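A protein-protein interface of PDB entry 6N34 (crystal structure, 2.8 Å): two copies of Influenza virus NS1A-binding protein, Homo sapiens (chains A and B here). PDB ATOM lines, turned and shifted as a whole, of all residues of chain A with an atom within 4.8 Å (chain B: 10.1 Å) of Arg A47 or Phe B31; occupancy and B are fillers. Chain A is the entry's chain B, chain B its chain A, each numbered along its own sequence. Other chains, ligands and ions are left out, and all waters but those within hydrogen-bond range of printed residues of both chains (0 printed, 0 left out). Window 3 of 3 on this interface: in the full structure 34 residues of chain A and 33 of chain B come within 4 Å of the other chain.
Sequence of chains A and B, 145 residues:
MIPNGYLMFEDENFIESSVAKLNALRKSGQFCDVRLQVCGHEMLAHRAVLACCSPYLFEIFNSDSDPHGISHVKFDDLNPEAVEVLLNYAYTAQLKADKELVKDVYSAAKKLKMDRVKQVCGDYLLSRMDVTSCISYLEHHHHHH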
ATOM      1  N   ASP A  33       6.035  14.279   1.181  1.00  0.00           N
ATOM      2  CA  ASP A  33       6.538  12.943   0.880  1.00  0.00           C
ATOM      3  C   ASP A  33       7.793  12.964   0.023  1.00  0.00           C
ATOM      4  O   ASP A  33       8.071  11.978  -0.665  1.00  0.00           O
ATOM      5  CB  ASP A  33       5.464  12.090   0.201  1.00  0.00           C
ATOM      6  CG  ASP A  33       4.585  12.882  -0.728  1.00  0.00           C
ATOM      7  OD1 ASP A  33       4.952  14.040  -1.038  1.00  0.00           O
ATOM      8  OD2 ASP A  33       3.524  12.353  -1.141  1.00  0.00           O
ATOM      9  N   VAL A  34       8.543  14.068   0.039  1.00  0.00           N
ATOM     10  CA  VAL A  34       9.827  14.185  -0.654  1.00  0.00           C
ATOM     11  C   VAL A  34      10.823  14.888   0.257  1.00  0.00           C
ATOM     12  O   VAL A  34      10.494  15.886   0.903  1.00  0.00           O
ATOM     13  CB  VAL A  34       9.713  14.962  -1.986  1.00  0.00           C
ATOM     14  CG1 VAL A  34      10.952  14.742  -2.826  1.00  0.00           C
ATOM     15  CG2 VAL A  34       8.504  14.551  -2.745  1.00  0.00           C
ATOM     16  N   ALA A  45       8.909  18.763   0.340  1.00  0.00           N
ATOM     17  CA  ALA A  45       7.973  19.122  -0.720  1.00  0.00           C
ATOM     18  C   ALA A  45       6.980  17.979  -0.909  1.00  0.00           C
ATOM     19  O   ALA A  45       7.124  16.901  -0.321  1.00  0.00           O
ATOM     20  CB  ALA A  45       8.719  19.434  -2.013  1.00  0.00           C
ATOM     21  N   HIS A  46       5.971  18.221  -1.744  1.00  0.00           N
ATOM     22  CA  HIS A  46       4.955  17.228  -2.071  1.00  0.00           C
ATOM     23  C   HIS A  46       5.176  16.728  -3.494  1.00  0.00           C
ATOM     24  O   HIS A  46       5.384  17.538  -4.402  1.00  0.00           O
ATOM     25  CB  HIS A  46       3.552  17.825  -1.925  1.00  0.00           C
ATOM     26  CG  HIS A  46       3.336  18.543  -0.629  1.00  0.00           C
ATOM     27  ND1 HIS A  46       3.723  19.850  -0.432  1.00  0.00           N
ATOM     28  CD2 HIS A  46       2.794  18.127   0.542  1.00  0.00           C
ATOM     29  CE1 HIS A  46       3.419  20.215   0.804  1.00  0.00           C
ATOM     30  NE2 HIS A  46       2.856  19.187   1.415  1.00  0.00           N
ATOM     31  N   ARG A  47       5.142  15.401  -3.690  1.00  0.00           N
ATOM     32  CA  ARG A  47       5.381  14.839  -5.020  1.00  0.00           C
ATOM     33  C   ARG A  47       4.414  15.413  -6.043  1.00  0.00           C
ATOM     34  O   ARG A  47       4.804  15.764  -7.164  1.00  0.00           O
ATOM     35  CB  ARG A  47       5.232  13.321  -5.018  1.00  0.00           C
ATOM     36  CG  ARG A  47       6.099  12.584  -4.070  1.00  0.00           C
ATOM     37  CD  ARG A  47       5.431  11.297  -3.626  1.00  0.00           C
ATOM     38  NE  ARG A  47       5.581  10.241  -4.610  1.00  0.00           N
ATOM     39  CZ  ARG A  47       4.984   9.055  -4.529  1.00  0.00           C
ATOM     40  NH1 ARG A  47       4.176   8.756  -3.502  1.00  0.00           N
ATOM     41  NH2 ARG A  47       5.204   8.155  -5.482  1.00  0.00           N
ATOM     42  N   ALA A  48       3.138  15.478  -5.682  1.00  0.00           N
ATOM     43  CA  ALA A  48       2.137  15.847  -6.663  1.00  0.00           C
ATOM     44  C   ALA A  48       2.408  17.234  -7.211  1.00  0.00           C
ATOM     45  O   ALA A  48       2.189  17.487  -8.406  1.00  0.00           O
ATOM     46  CB  ALA A  48       0.743  15.764  -6.050  1.00  0.00           C
ATOM     47  N   VAL A  49       2.903  18.140  -6.376  1.00  0.00           N
ATOM     48  CA  VAL A  49       3.331  19.436  -6.894  1.00  0.00           C
ATOM     49  C   VAL A  49       4.497  19.250  -7.877  1.00  0.00           C
ATOM     50  O   VAL A  49       4.365  19.485  -9.081  1.00  0.00           O
ATOM     51  CB  VAL A  49       3.694  20.386  -5.746  1.00  0.00           C
ATOM     52  CG1 VAL A  49       3.901  21.807  -6.282  1.00  0.00           C
ATOM     53  CG2 VAL A  49       2.617  20.368  -4.693  1.00  0.00           C
ATOM     54  N   LEU A  50       5.624  18.759  -7.371  1.00  0.00           N
ATOM     55  CA  LEU A  50       6.832  18.684  -8.187  1.00  0.00           C
ATOM     56  C   LEU A  50       6.650  17.894  -9.485  1.00  0.00           C
ATOM     57  O   LEU A  50       7.365  18.158 -10.463  1.00  0.00           O
ATOM     58  CB  LEU A  50       7.962  18.093  -7.345  1.00  0.00           C
ATOM     59  CG  LEU A  50       8.154  18.795  -5.997  1.00  0.00           C
ATOM     60  CD1 LEU A  50       9.345  18.241  -5.301  1.00  0.00           C
ATOM     61  CD2 LEU A  50       8.324  20.283  -6.156  1.00  0.00           C
ATOM     62  N   ALA A  51       5.728  16.929  -9.516  1.00  0.00           N
ATOM     63  CA  ALA A  51       5.520  16.160 -10.735  1.00  0.00           C
ATOM     64  C   ALA A  51       4.836  16.996 -11.812  1.00  0.00           C
ATOM     65  O   ALA A  51       5.176  16.883 -12.993  1.00  0.00           O
ATOM     66  CB  ALA A  51       4.724  14.892 -10.422  1.00  0.00           C
ATOM     67  N   PHE A  58       8.965  13.843 -12.191  1.00  0.00           N
ATOM     68  CA  PHE A  58       7.898  12.910 -12.523  1.00  0.00           C
ATOM     69  C   PHE A  58       8.472  11.530 -12.804  1.00  0.00           C
ATOM     70  O   PHE A  58       8.012  10.526 -12.254  1.00  0.00           O
ATOM     71  CB  PHE A  58       7.119  13.430 -13.728  1.00  0.00           C
ATOM     72  CG  PHE A  58       5.727  12.904 -13.820  1.00  0.00           C
ATOM     73  CD1 PHE A  58       5.319  11.847 -13.020  1.00  0.00           C
ATOM     74  CD2 PHE A  58       4.816  13.473 -14.707  1.00  0.00           C
ATOM     75  CE1 PHE A  58       4.027  11.352 -13.097  1.00  0.00           C
ATOM     76  CE2 PHE A  58       3.516  12.995 -14.790  1.00  0.00           C
ATOM     77  CZ  PHE A  58       3.120  11.922 -13.980  1.00  0.00           C
ATOM     78  N   PHE A  61       9.784   9.782  -9.925  1.00  0.00           N
ATOM     79  CA  PHE A  61       8.808   9.473  -8.867  1.00  0.00           C
ATOM     80  C   PHE A  61       7.983   8.301  -9.322  1.00  0.00           C
ATOM     81  O   PHE A  61       7.569   7.511  -8.496  1.00  0.00           O
ATOM     82  CB  PHE A  61       7.795  10.594  -8.731  1.00  0.00           C
ATOM     83  CG  PHE A  61       8.292  11.750  -7.921  1.00  0.00           C
ATOM     84  CD1 PHE A  61       9.358  11.595  -7.075  1.00  0.00           C
ATOM     85  CD2 PHE A  61       7.707  12.986  -8.028  1.00  0.00           C
ATOM     86  CE1 PHE A  61       9.824  12.662  -6.337  1.00  0.00           C
ATOM     87  CE2 PHE A  61       8.178  14.051  -7.295  1.00  0.00           C
ATOM     88  CZ  PHE A  61       9.236  13.885  -6.452  1.00  0.00           C
ATOM     89  N   ASN A  62       7.710   8.237 -10.606  1.00  0.00           N
ATOM     90  CA  ASN A  62       6.896   7.084 -11.035  1.00  0.00           C
ATOM     91  C   ASN A  62       7.856   5.902 -11.158  1.00  0.00           C
ATOM     92  O   ASN A  62       8.608   5.889 -12.127  1.00  0.00           O
ATOM     93  CB  ASN A  62       6.104   7.448 -12.284  1.00  0.00           C
ATOM     94  CG  ASN A  62       5.653   6.249 -13.081  1.00  0.00           C
ATOM     95  OD1 ASN A  62       5.751   5.108 -12.627  1.00  0.00           O
ATOM     96  ND2 ASN A  62       5.147   6.509 -14.274  1.00  0.00           N
ATOM     97  N   SER A  71       9.932   9.679  -0.846  1.00  0.00           N
ATOM     98  CA  SER A  71      10.898   9.733  -1.942  1.00  0.00           C
ATOM     99  C   SER A  71      12.087  10.607  -1.550  1.00  0.00           C
ATOM    100  O   SER A  71      11.909  11.778  -1.202  1.00  0.00           O
ATOM    101  CB  SER A  71      10.243  10.259  -3.223  1.00  0.00           C
ATOM    102  OG  SER A  71       9.236   9.370  -3.702  1.00  0.00           O
ATOM    103  N   SER B  18      -1.566  23.455 -13.971  1.00  0.00           N
ATOM    104  CA  SER B  18      -1.177  22.483 -12.964  1.00  0.00           C
ATOM    105  C   SER B  18      -2.335  22.021 -12.091  1.00  0.00           C
ATOM    106  O   SER B  18      -2.289  20.890 -11.596  1.00  0.00           O
ATOM    107  CB  SER B  18      -0.032  23.033 -12.095  1.00  0.00           C
ATOM    108  OG  SER B  18      -0.318  24.312 -11.556  1.00  0.00           O
ATOM    109  N   LYS B  21      -3.245  19.442 -14.271  1.00  0.00           N
ATOM    110  CA  LYS B  21      -2.328  18.299 -14.140  1.00  0.00           C
ATOM    111  C   LYS B  21      -2.660  17.631 -12.823  1.00  0.00           C
ATOM    112  O   LYS B  21      -2.832  16.440 -12.817  1.00  0.00           O
ATOM    113  CB  LYS B  21      -0.877  18.765 -14.191  1.00  0.00           C
ATOM    114  CG  LYS B  21      -0.424  19.313 -15.530  1.00  0.00           C
ATOM    115  CD  LYS B  21       1.056  19.187 -15.750  1.00  0.00           C
ATOM    116  CE  LYS B  21       1.524  19.863 -17.017  1.00  0.00           C
ATOM    117  NZ  LYS B  21       2.123  21.187 -16.739  1.00  0.00           N
ATOM    118  N   LEU B  22      -2.799  18.402 -11.763  1.00  0.00           N
ATOM    119  CA  LEU B  22      -3.108  17.775 -10.466  1.00  0.00           C
ATOM    120  C   LEU B  22      -4.440  17.068 -10.566  1.00  0.00           C
ATOM    121  O   LEU B  22      -4.553  15.966 -10.127  1.00  0.00           O
ATOM    122  CB  LEU B  22      -3.169  18.855  -9.403  1.00  0.00           C
ATOM    123  CG  LEU B  22      -2.065  18.707  -8.384  1.00  0.00           C
ATOM    124  CD1 LEU B  22      -1.849  19.990  -7.642  1.00  0.00           C
ATOM    125  CD2 LEU B  22      -2.401  17.590  -7.447  1.00  0.00           C
ATOM    126  N   ALA B  24      -5.803  15.797 -13.138  1.00  0.00           N
ATOM    127  CA  ALA B  24      -5.461  14.626 -13.935  1.00  0.00           C
ATOM    128  C   ALA B  24      -4.836  13.527 -13.070  1.00  0.00           C
ATOM    129  O   ALA B  24      -5.185  12.346 -13.200  1.00  0.00           O
ATOM    130  CB  ALA B  24      -4.524  15.029 -15.068  1.00  0.00           C
ATOM    131  N   LEU B  25      -3.920  13.908 -12.167  1.00  0.00           N
ATOM    132  CA  LEU B  25      -3.285  12.941 -11.267  1.00  0.00           C
ATOM    133  C   LEU B  25      -4.311  12.213 -10.410  1.00  0.00           C
ATOM    134  O   LEU B  25      -4.310  10.976 -10.333  1.00  0.00           O
ATOM    135  CB  LEU B  25      -2.276  13.635 -10.357  1.00  0.00           C
ATOM    136  CG  LEU B  25      -0.930  13.938 -11.004  1.00  0.00           C
ATOM    137  CD1 LEU B  25       0.099  14.291  -9.936  1.00  0.00           C
ATOM    138  CD2 LEU B  25      -0.476  12.757 -11.870  1.00  0.00           C
ATOM    139  N   ARG B  26      -5.181  12.975  -9.737  1.00  0.00           N
ATOM    140  CA  ARG B  26      -6.182  12.374  -8.864  1.00  0.00           C
ATOM    141  C   ARG B  26      -7.059  11.385  -9.623  1.00  0.00           C
ATOM    142  O   ARG B  26      -7.296  10.272  -9.147  1.00  0.00           O
ATOM    143  CB  ARG B  26      -7.026  13.464  -8.212  1.00  0.00           C
ATOM    144  CG  ARG B  26      -8.084  12.923  -7.274  1.00  0.00           C
ATOM    145  CD  ARG B  26      -9.070  13.997  -6.854  1.00  0.00           C
ATOM    146  NE  ARG B  26      -9.704  14.624  -8.007  1.00  0.00           N
ATOM    147  CZ  ARG B  26     -10.946  14.370  -8.390  1.00  0.00           C
ATOM    148  NH1 ARG B  26     -11.684  13.511  -7.689  1.00  0.00           N
ATOM    149  NH2 ARG B  26     -11.449  14.976  -9.461  1.00  0.00           N
ATOM    150  N   LYS B  27      -7.516  11.752 -10.820  1.00  0.00           N
ATOM    151  CA  LYS B  27      -8.376  10.870 -11.600  1.00  0.00           C
ATOM    152  C   LYS B  27      -7.625   9.692 -12.216  1.00  0.00           C
ATOM    153  O   LYS B  27      -8.261   8.812 -12.805  1.00  0.00           O
ATOM    154  CB  LYS B  27      -9.079  11.688 -12.681  1.00  0.00           C
ATOM    155  CG  LYS B  27     -10.024  12.763 -12.110  1.00  0.00           C
ATOM    156  CD  LYS B  27     -10.332  13.831 -13.135  1.00  0.00           C
ATOM    157  CE  LYS B  27     -11.730  14.399 -12.957  1.00  0.00           C
ATOM    158  NZ  LYS B  27     -12.108  15.265 -14.124  1.00  0.00           N
ATOM    159  N   SER B  28      -6.296   9.650 -12.091  1.00  0.00           N
ATOM    160  CA  SER B  28      -5.482   8.537 -12.558  1.00  0.00           C
ATOM    161  C   SER B  28      -4.886   7.740 -11.411  1.00  0.00           C
ATOM    162  O   SER B  28      -4.166   6.761 -11.659  1.00  0.00           O
ATOM    163  CB  SER B  28      -4.359   9.052 -13.456  1.00  0.00           C
ATOM    164  OG  SER B  28      -3.754  10.184 -12.870  1.00  0.00           O
ATOM    165  N   GLY B  29      -5.157   8.144 -10.174  1.00  0.00           N
ATOM    166  CA  GLY B  29      -4.617   7.485  -8.996  1.00  0.00           C
ATOM    167  C   GLY B  29      -3.111   7.520  -8.870  1.00  0.00           C
ATOM    168  O   GLY B  29      -2.496   6.488  -8.580  1.00  0.00           O
ATOM    169  N   GLN B  30      -2.498   8.680  -9.062  1.00  0.00           N
ATOM    170  CA  GLN B  30      -1.051   8.797  -8.991  1.00  0.00           C
ATOM    171  C   GLN B  30      -0.638   9.633  -7.793  1.00  0.00           C
ATOM    172  O   GLN B  30      -1.141  10.744  -7.596  1.00  0.00           O
ATOM    173  CB  GLN B  30      -0.489   9.401 -10.269  1.00  0.00           C
ATOM    174  CG  GLN B  30      -0.499   8.426 -11.412  1.00  0.00           C
ATOM    175  CD  GLN B  30       0.366   8.899 -12.550  1.00  0.00           C
ATOM    176  OE1 GLN B  30       1.535   8.512 -12.651  1.00  0.00           O
ATOM    177  NE2 GLN B  30      -0.193   9.745 -13.413  1.00  0.00           N
ATOM    178  N   PHE B  31       0.284   9.089  -7.006  1.00  0.00           N
ATOM    179  CA  PHE B  31       0.862   9.754  -5.847  1.00  0.00           C
ATOM    180  C   PHE B  31      -0.172  10.036  -4.764  1.00  0.00           C
ATOM    181  O   PHE B  31       0.097  10.798  -3.834  1.00  0.00           O
ATOM    182  CB  PHE B  31       1.582  11.058  -6.234  1.00  0.00           C
ATOM    183  CG  PHE B  31       2.503  10.918  -7.399  1.00  0.00           C
ATOM    184  CD1 PHE B  31       3.572  10.052  -7.346  1.00  0.00           C
ATOM    185  CD2 PHE B  31       2.302  11.650  -8.555  1.00  0.00           C
ATOM    186  CE1 PHE B  31       4.419   9.913  -8.429  1.00  0.00           C
ATOM    187  CE2 PHE B  31       3.158  11.514  -9.641  1.00  0.00           C
ATOM    188  CZ  PHE B  31       4.215  10.654  -9.576  1.00  0.00           C
ATOM    189  N   CYS B  32      -1.347   9.425  -4.827  1.00  0.00           N
ATOM    190  CA  CYS B  32      -2.343   9.711  -3.804  1.00  0.00           C
ATOM    191  C   CYS B  32      -1.966   9.060  -2.472  1.00  0.00           C
ATOM    192  O   CYS B  32      -1.225   8.077  -2.410  1.00  0.00           O
ATOM    193  CB  CYS B  32      -3.723   9.246  -4.261  1.00  0.00           C
ATOM    194  SG  CYS B  32      -4.355  10.137  -5.730  1.00  0.00           S
ATOM    195  N   ASP B  33      -2.480   9.641  -1.390  1.00  0.00           N
ATOM    196  CA  ASP B  33      -2.176   9.148  -0.055  1.00  0.00           C
ATOM    197  C   ASP B  33      -3.391   9.210   0.864  1.00  0.00           C
ATOM    198  O   ASP B  33      -3.244   9.043   2.080  1.00  0.00           O
ATOM    199  CB  ASP B  33      -0.992   9.918   0.552  1.00  0.00           C
ATOM    200  CG  ASP B  33      -1.228  11.427   0.625  1.00  0.00           C
ATOM    201  OD1 ASP B  33      -2.177  11.940  -0.021  1.00  0.00           O
ATOM    202  OD2 ASP B  33      -0.457  12.102   1.344  1.00  0.00           O
ATOM    203  N   VAL B  34      -4.574   9.462   0.321  1.00  0.00           N
ATOM    204  CA  VAL B  34      -5.841   9.302   1.021  1.00  0.00           C
ATOM    205  C   VAL B  34      -6.741   8.423   0.177  1.00  0.00           C
ATOM    206  O   VAL B  34      -6.816   8.596  -1.049  1.00  0.00           O
ATOM    207  CB  VAL B  34      -6.550  10.644   1.286  1.00  0.00           C
ATOM    208  CG1 VAL B  34      -7.337  10.557   2.587  1.00  0.00           C
ATOM    209  CG2 VAL B  34      -5.568  11.778   1.291  1.00  0.00           C
ATOM    210  N   ARG B  35      -7.429   7.484   0.827  1.00  0.00           N
ATOM    211  CA  ARG B  35      -8.499   6.703   0.216  1.00  0.00           C
ATOM    212  C   ARG B  35      -9.793   7.064   0.929  1.00  0.00           C
ATOM    213  O   ARG B  35      -9.948   6.785   2.122  1.00  0.00           O
ATOM    214  CB  ARG B  35      -8.225   5.207   0.310  1.00  0.00           C
ATOM    215  CG  ARG B  35      -6.998   4.745  -0.445  1.00  0.00           C
ATOM    216  CD  ARG B  35      -6.736   3.272  -0.176  1.00  0.00           C
ATOM    217  NE  ARG B  35      -7.925   2.447  -0.387  1.00  0.00           N
ATOM    218  CZ  ARG B  35      -7.918   1.116  -0.381  1.00  0.00           C
ATOM    219  NH1 ARG B  35      -6.780   0.456  -0.176  1.00  0.00           N
ATOM    220  NH2 ARG B  35      -9.047   0.443  -0.583  1.00  0.00           N
ATOM    221  N   LEU B  44      -9.627   8.192  -4.429  1.00  0.00           N
ATOM    222  CA  LEU B  44      -8.351   8.595  -3.828  1.00  0.00           C
ATOM    223  C   LEU B  44      -8.125  10.067  -4.063  1.00  0.00           C
ATOM    224  O   LEU B  44      -8.748  10.614  -4.931  1.00  0.00           O
ATOM    225  CB  LEU B  44      -7.260   7.782  -4.500  1.00  0.00           C
ATOM    226  CG  LEU B  44      -7.727   6.408  -4.927  1.00  0.00           C
ATOM    227  CD1 LEU B  44      -6.733   5.793  -5.876  1.00  0.00           C
ATOM    228  CD2 LEU B  44      -7.902   5.539  -3.712  1.00  0.00           C
ATOM    229  N   ALA B  45      -7.215  10.633  -3.296  1.00  0.00           N
ATOM    230  CA  ALA B  45      -6.884  12.057  -3.382  1.00  0.00           C
ATOM    231  C   ALA B  45      -5.558  12.303  -2.689  1.00  0.00           C
ATOM    232  O   ALA B  45      -4.944  11.380  -2.238  1.00  0.00           O
ATOM    233  CB  ALA B  45      -7.968  12.820  -2.707  1.00  0.00           C
ATOM    234  N   HIS B  46      -5.149  13.549  -2.614  1.00  0.00           N
ATOM    235  CA  HIS B  46      -3.884  13.885  -1.960  1.00  0.00           C
ATOM    236  C   HIS B  46      -4.151  14.575  -0.630  1.00  0.00           C
ATOM    237  O   HIS B  46      -4.936  15.529  -0.562  1.00  0.00           O
ATOM    238  CB  HIS B  46      -3.020  14.767  -2.863  1.00  0.00           C
ATOM    239  CG  HIS B  46      -2.790  14.170  -4.213  1.00  0.00           C
ATOM    240  ND1 HIS B  46      -3.520  14.539  -5.323  1.00  0.00           N
ATOM    241  CD2 HIS B  46      -1.942  13.192  -4.625  1.00  0.00           C
ATOM    242  CE1 HIS B  46      -3.121  13.824  -6.367  1.00  0.00           C
ATOM    243  NE2 HIS B  46      -2.169  12.996  -5.968  1.00  0.00           N
ATOM    244  N   ARG B  47      -3.515  14.066   0.427  1.00  0.00           N
ATOM    245  CA  ARG B  47      -3.654  14.661   1.751  1.00  0.00           C
ATOM    246  C   ARG B  47      -3.504  16.168   1.689  1.00  0.00           C
ATOM    247  O   ARG B  47      -4.318  16.911   2.243  1.00  0.00           O
ATOM    248  CB  ARG B  47      -2.606  14.088   2.692  1.00  0.00           C
ATOM    249  CG  ARG B  47      -3.089  13.025   3.600  1.00  0.00           C
ATOM    250  CD  ARG B  47      -1.924  12.483   4.396  1.00  0.00           C
ATOM    251  NE  ARG B  47      -1.992  11.030   4.480  1.00  0.00           N
ATOM    252  CZ  ARG B  47      -0.946  10.253   4.735  1.00  0.00           C
ATOM    253  NH1 ARG B  47       0.245  10.802   4.925  1.00  0.00           N
ATOM    254  NH2 ARG B  47      -1.085   8.936   4.801  1.00  0.00           N
ATOM    255  N   ALA B  48      -2.453  16.635   1.011  1.00  0.00           N
ATOM    256  CA  ALA B  48      -2.115  18.052   1.052  1.00  0.00           C
ATOM    257  C   ALA B  48      -3.210  18.893   0.424  1.00  0.00           C
ATOM    258  O   ALA B  48      -3.608  19.916   0.994  1.00  0.00           O
ATOM    259  CB  ALA B  48      -0.783  18.297   0.354  1.00  0.00           C
ATOM    260  N   VAL B  49      -3.731  18.463  -0.734  1.00  0.00           N
ATOM    261  CA  VAL B  49      -4.810  19.210  -1.395  1.00  0.00           C
ATOM    262  C   VAL B  49      -6.049  19.260  -0.508  1.00  0.00           C
ATOM    263  O   VAL B  49      -6.576  20.339  -0.220  1.00  0.00           O
ATOM    264  CB  VAL B  49      -5.136  18.605  -2.773  1.00  0.00           C
ATOM    265  CG1 VAL B  49      -6.276  19.366  -3.429  1.00  0.00           C
ATOM    266  CG2 VAL B  49      -3.892  18.576  -3.654  1.00  0.00           C
ATOM    267  N   ILE B  70      -0.659   4.909   4.346  1.00  0.00           N
ATOM    268  CA  ILE B  70      -1.512   5.964   3.807  1.00  0.00           C
ATOM    269  C   ILE B  70      -2.869   5.951   4.512  1.00  0.00           C
ATOM    270  O   ILE B  70      -3.245   4.985   5.181  1.00  0.00           O
ATOM    271  CB  ILE B  70      -1.665   5.848   2.279  1.00  0.00           C
ATOM    272  CG1 ILE B  70      -2.619   4.712   1.892  1.00  0.00           C
ATOM    273  CG2 ILE B  70      -0.296   5.687   1.633  1.00  0.00           C
ATOM    274  CD1 ILE B  70      -3.047   4.746   0.436  1.00  0.00           C
ATOM    275  N   SER B  71      -3.610   7.049   4.363  1.00  0.00           N
ATOM    276  CA  SER B  71      -4.759   7.323   5.221  1.00  0.00           C
ATOM    277  C   SER B  71      -6.045   6.756   4.645  1.00  0.00           C
ATOM    278  O   SER B  71      -6.326   6.898   3.451  1.00  0.00           O
ATOM    279  CB  SER B  71      -4.934   8.827   5.439  1.00  0.00           C
ATOM    280  OG  SER B  71      -3.837   9.399   6.125  1.00  0.00           O
ATOM    281  N   TYR B  91      -9.927  20.549  -6.110  1.00  0.00           N
ATOM    282  CA  TYR B  91      -8.790  20.548  -7.012  1.00  0.00           C
ATOM    283  C   TYR B  91      -8.812  21.743  -7.945  1.00  0.00           C
ATOM    284  O   TYR B  91      -7.827  22.484  -8.027  1.00  0.00           O
ATOM    285  CB  TYR B  91      -8.745  19.237  -7.800  1.00  0.00           C
ATOM    286  CG  TYR B  91      -8.006  18.189  -7.024  1.00  0.00           C
ATOM    287  CD1 TYR B  91      -8.598  17.578  -5.930  1.00  0.00           C
ATOM    288  CD2 TYR B  91      -6.700  17.865  -7.332  1.00  0.00           C
ATOM    289  CE1 TYR B  91      -7.921  16.644  -5.178  1.00  0.00           C
ATOM    290  CE2 TYR B  91      -6.016  16.932  -6.597  1.00  0.00           C
ATOM    291  CZ  TYR B  91      -6.628  16.320  -5.518  1.00  0.00           C
ATOM    292  OH  TYR B  91      -5.942  15.387  -4.784  1.00  0.00           O
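The backbone carbonyl oxygen (O) of Leu B25 is in hydrogen-bond range of the backbone NH (N) of Gln B30, 3.2 Å away.
The side-chain sulfur (SG) of Cys B32 sits at hydrogen-bond distance from the backbone carbonyl oxygen (O) of Gln B30, 3.8 Å away.
O of Gln B30 sits at hydrogen-bond distance from NE2 of His B46 (3.0 Å).
The side-chain sulfur (SG) of Cys B32 is in hydrogen-bond range of a ring nitrogen (NE2) of His B46.
A ring nitrogen (ND1) of His B46 lies within hydrogen-bond range of the side-chain hydroxyl (OH) of Tyr B91.
OD1 of Asp A33 sits at hydrogen-bond distance from N of Arg A47, 3.0 Å away.
Among the printed residues, pairs that only touch across the chains: His A46 with Ala B48 (3.6 Å), Arg A47 with Phe B31 (3.1 Å), Ala A48 with Leu B22 (3.9 Å), Ala A48 with His B46 (3.98 Å), Ala A51 with Phe B31 (3.8 Å), Phe A58 with Gln B30 (3.8 Å), Phe A58 with Phe B31 (3.6 Å) and Phe A61 with Phe B31 (3.5 Å).
Of chain B, only Phe B31 (3.1 Å) comes within 4 Å of Arg A47.
Phe B31 touches just these residues of chain A: Arg A47 (3.1 Å), Ala A51 (3.8 Å), Phe A58 (3.6 Å) and Phe A61 (3.5 Å).
No residue of chain B comes within 4 Å of Asp A33.
No residue of chain B comes within 4 Å of Leu A50.
Ala A51 touches just one residue of chain B: Phe B31.
Of chain B, only Phe B31 (3.5 Å) comes within 4 Å of Phe A61.
Of the printed residues of chain B, Phe A58 touches Gln B30 (3.8 Å) and Phe B31 (3.6 Å).
Printed residues of chain B within 4 Å of His A46: Ala B48.
Of the printed residues of chain A, Gln B30 touches Phe A58.
Of the printed residues of chain A, His B46 touches Ala A48.
Ser B18 touches none of the printed residues of chain A.
Ile B70 touches none of the printed residues of chain A.
The nearest residue of chain B that does not touch Arg A47 is Cys B32 (5.6 Å).
The nearest printed residue of chain A that does not touch His B46 is Asp A33 (6.5 Å).
Hydrophobic or aromatic side chains of chain B that line the printed part of chain A: Leu B22, Phe B31, His B46 and Ala B48.
Of the 13 printed residues of chain A, 6 touch a printed residue of chain B.
Hydrophobic or aromatic side chains of chain A that line the printed part of chain B: His A46, Ala A48, Ala A51, Phe A58 and Phe A61.
His A46 touches Ala B48, and with the chains exchanged Ala A48 touches His B46.
Positions printed for both chains: 33, 34, 45, 46, 47, 48, 49 and 71.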
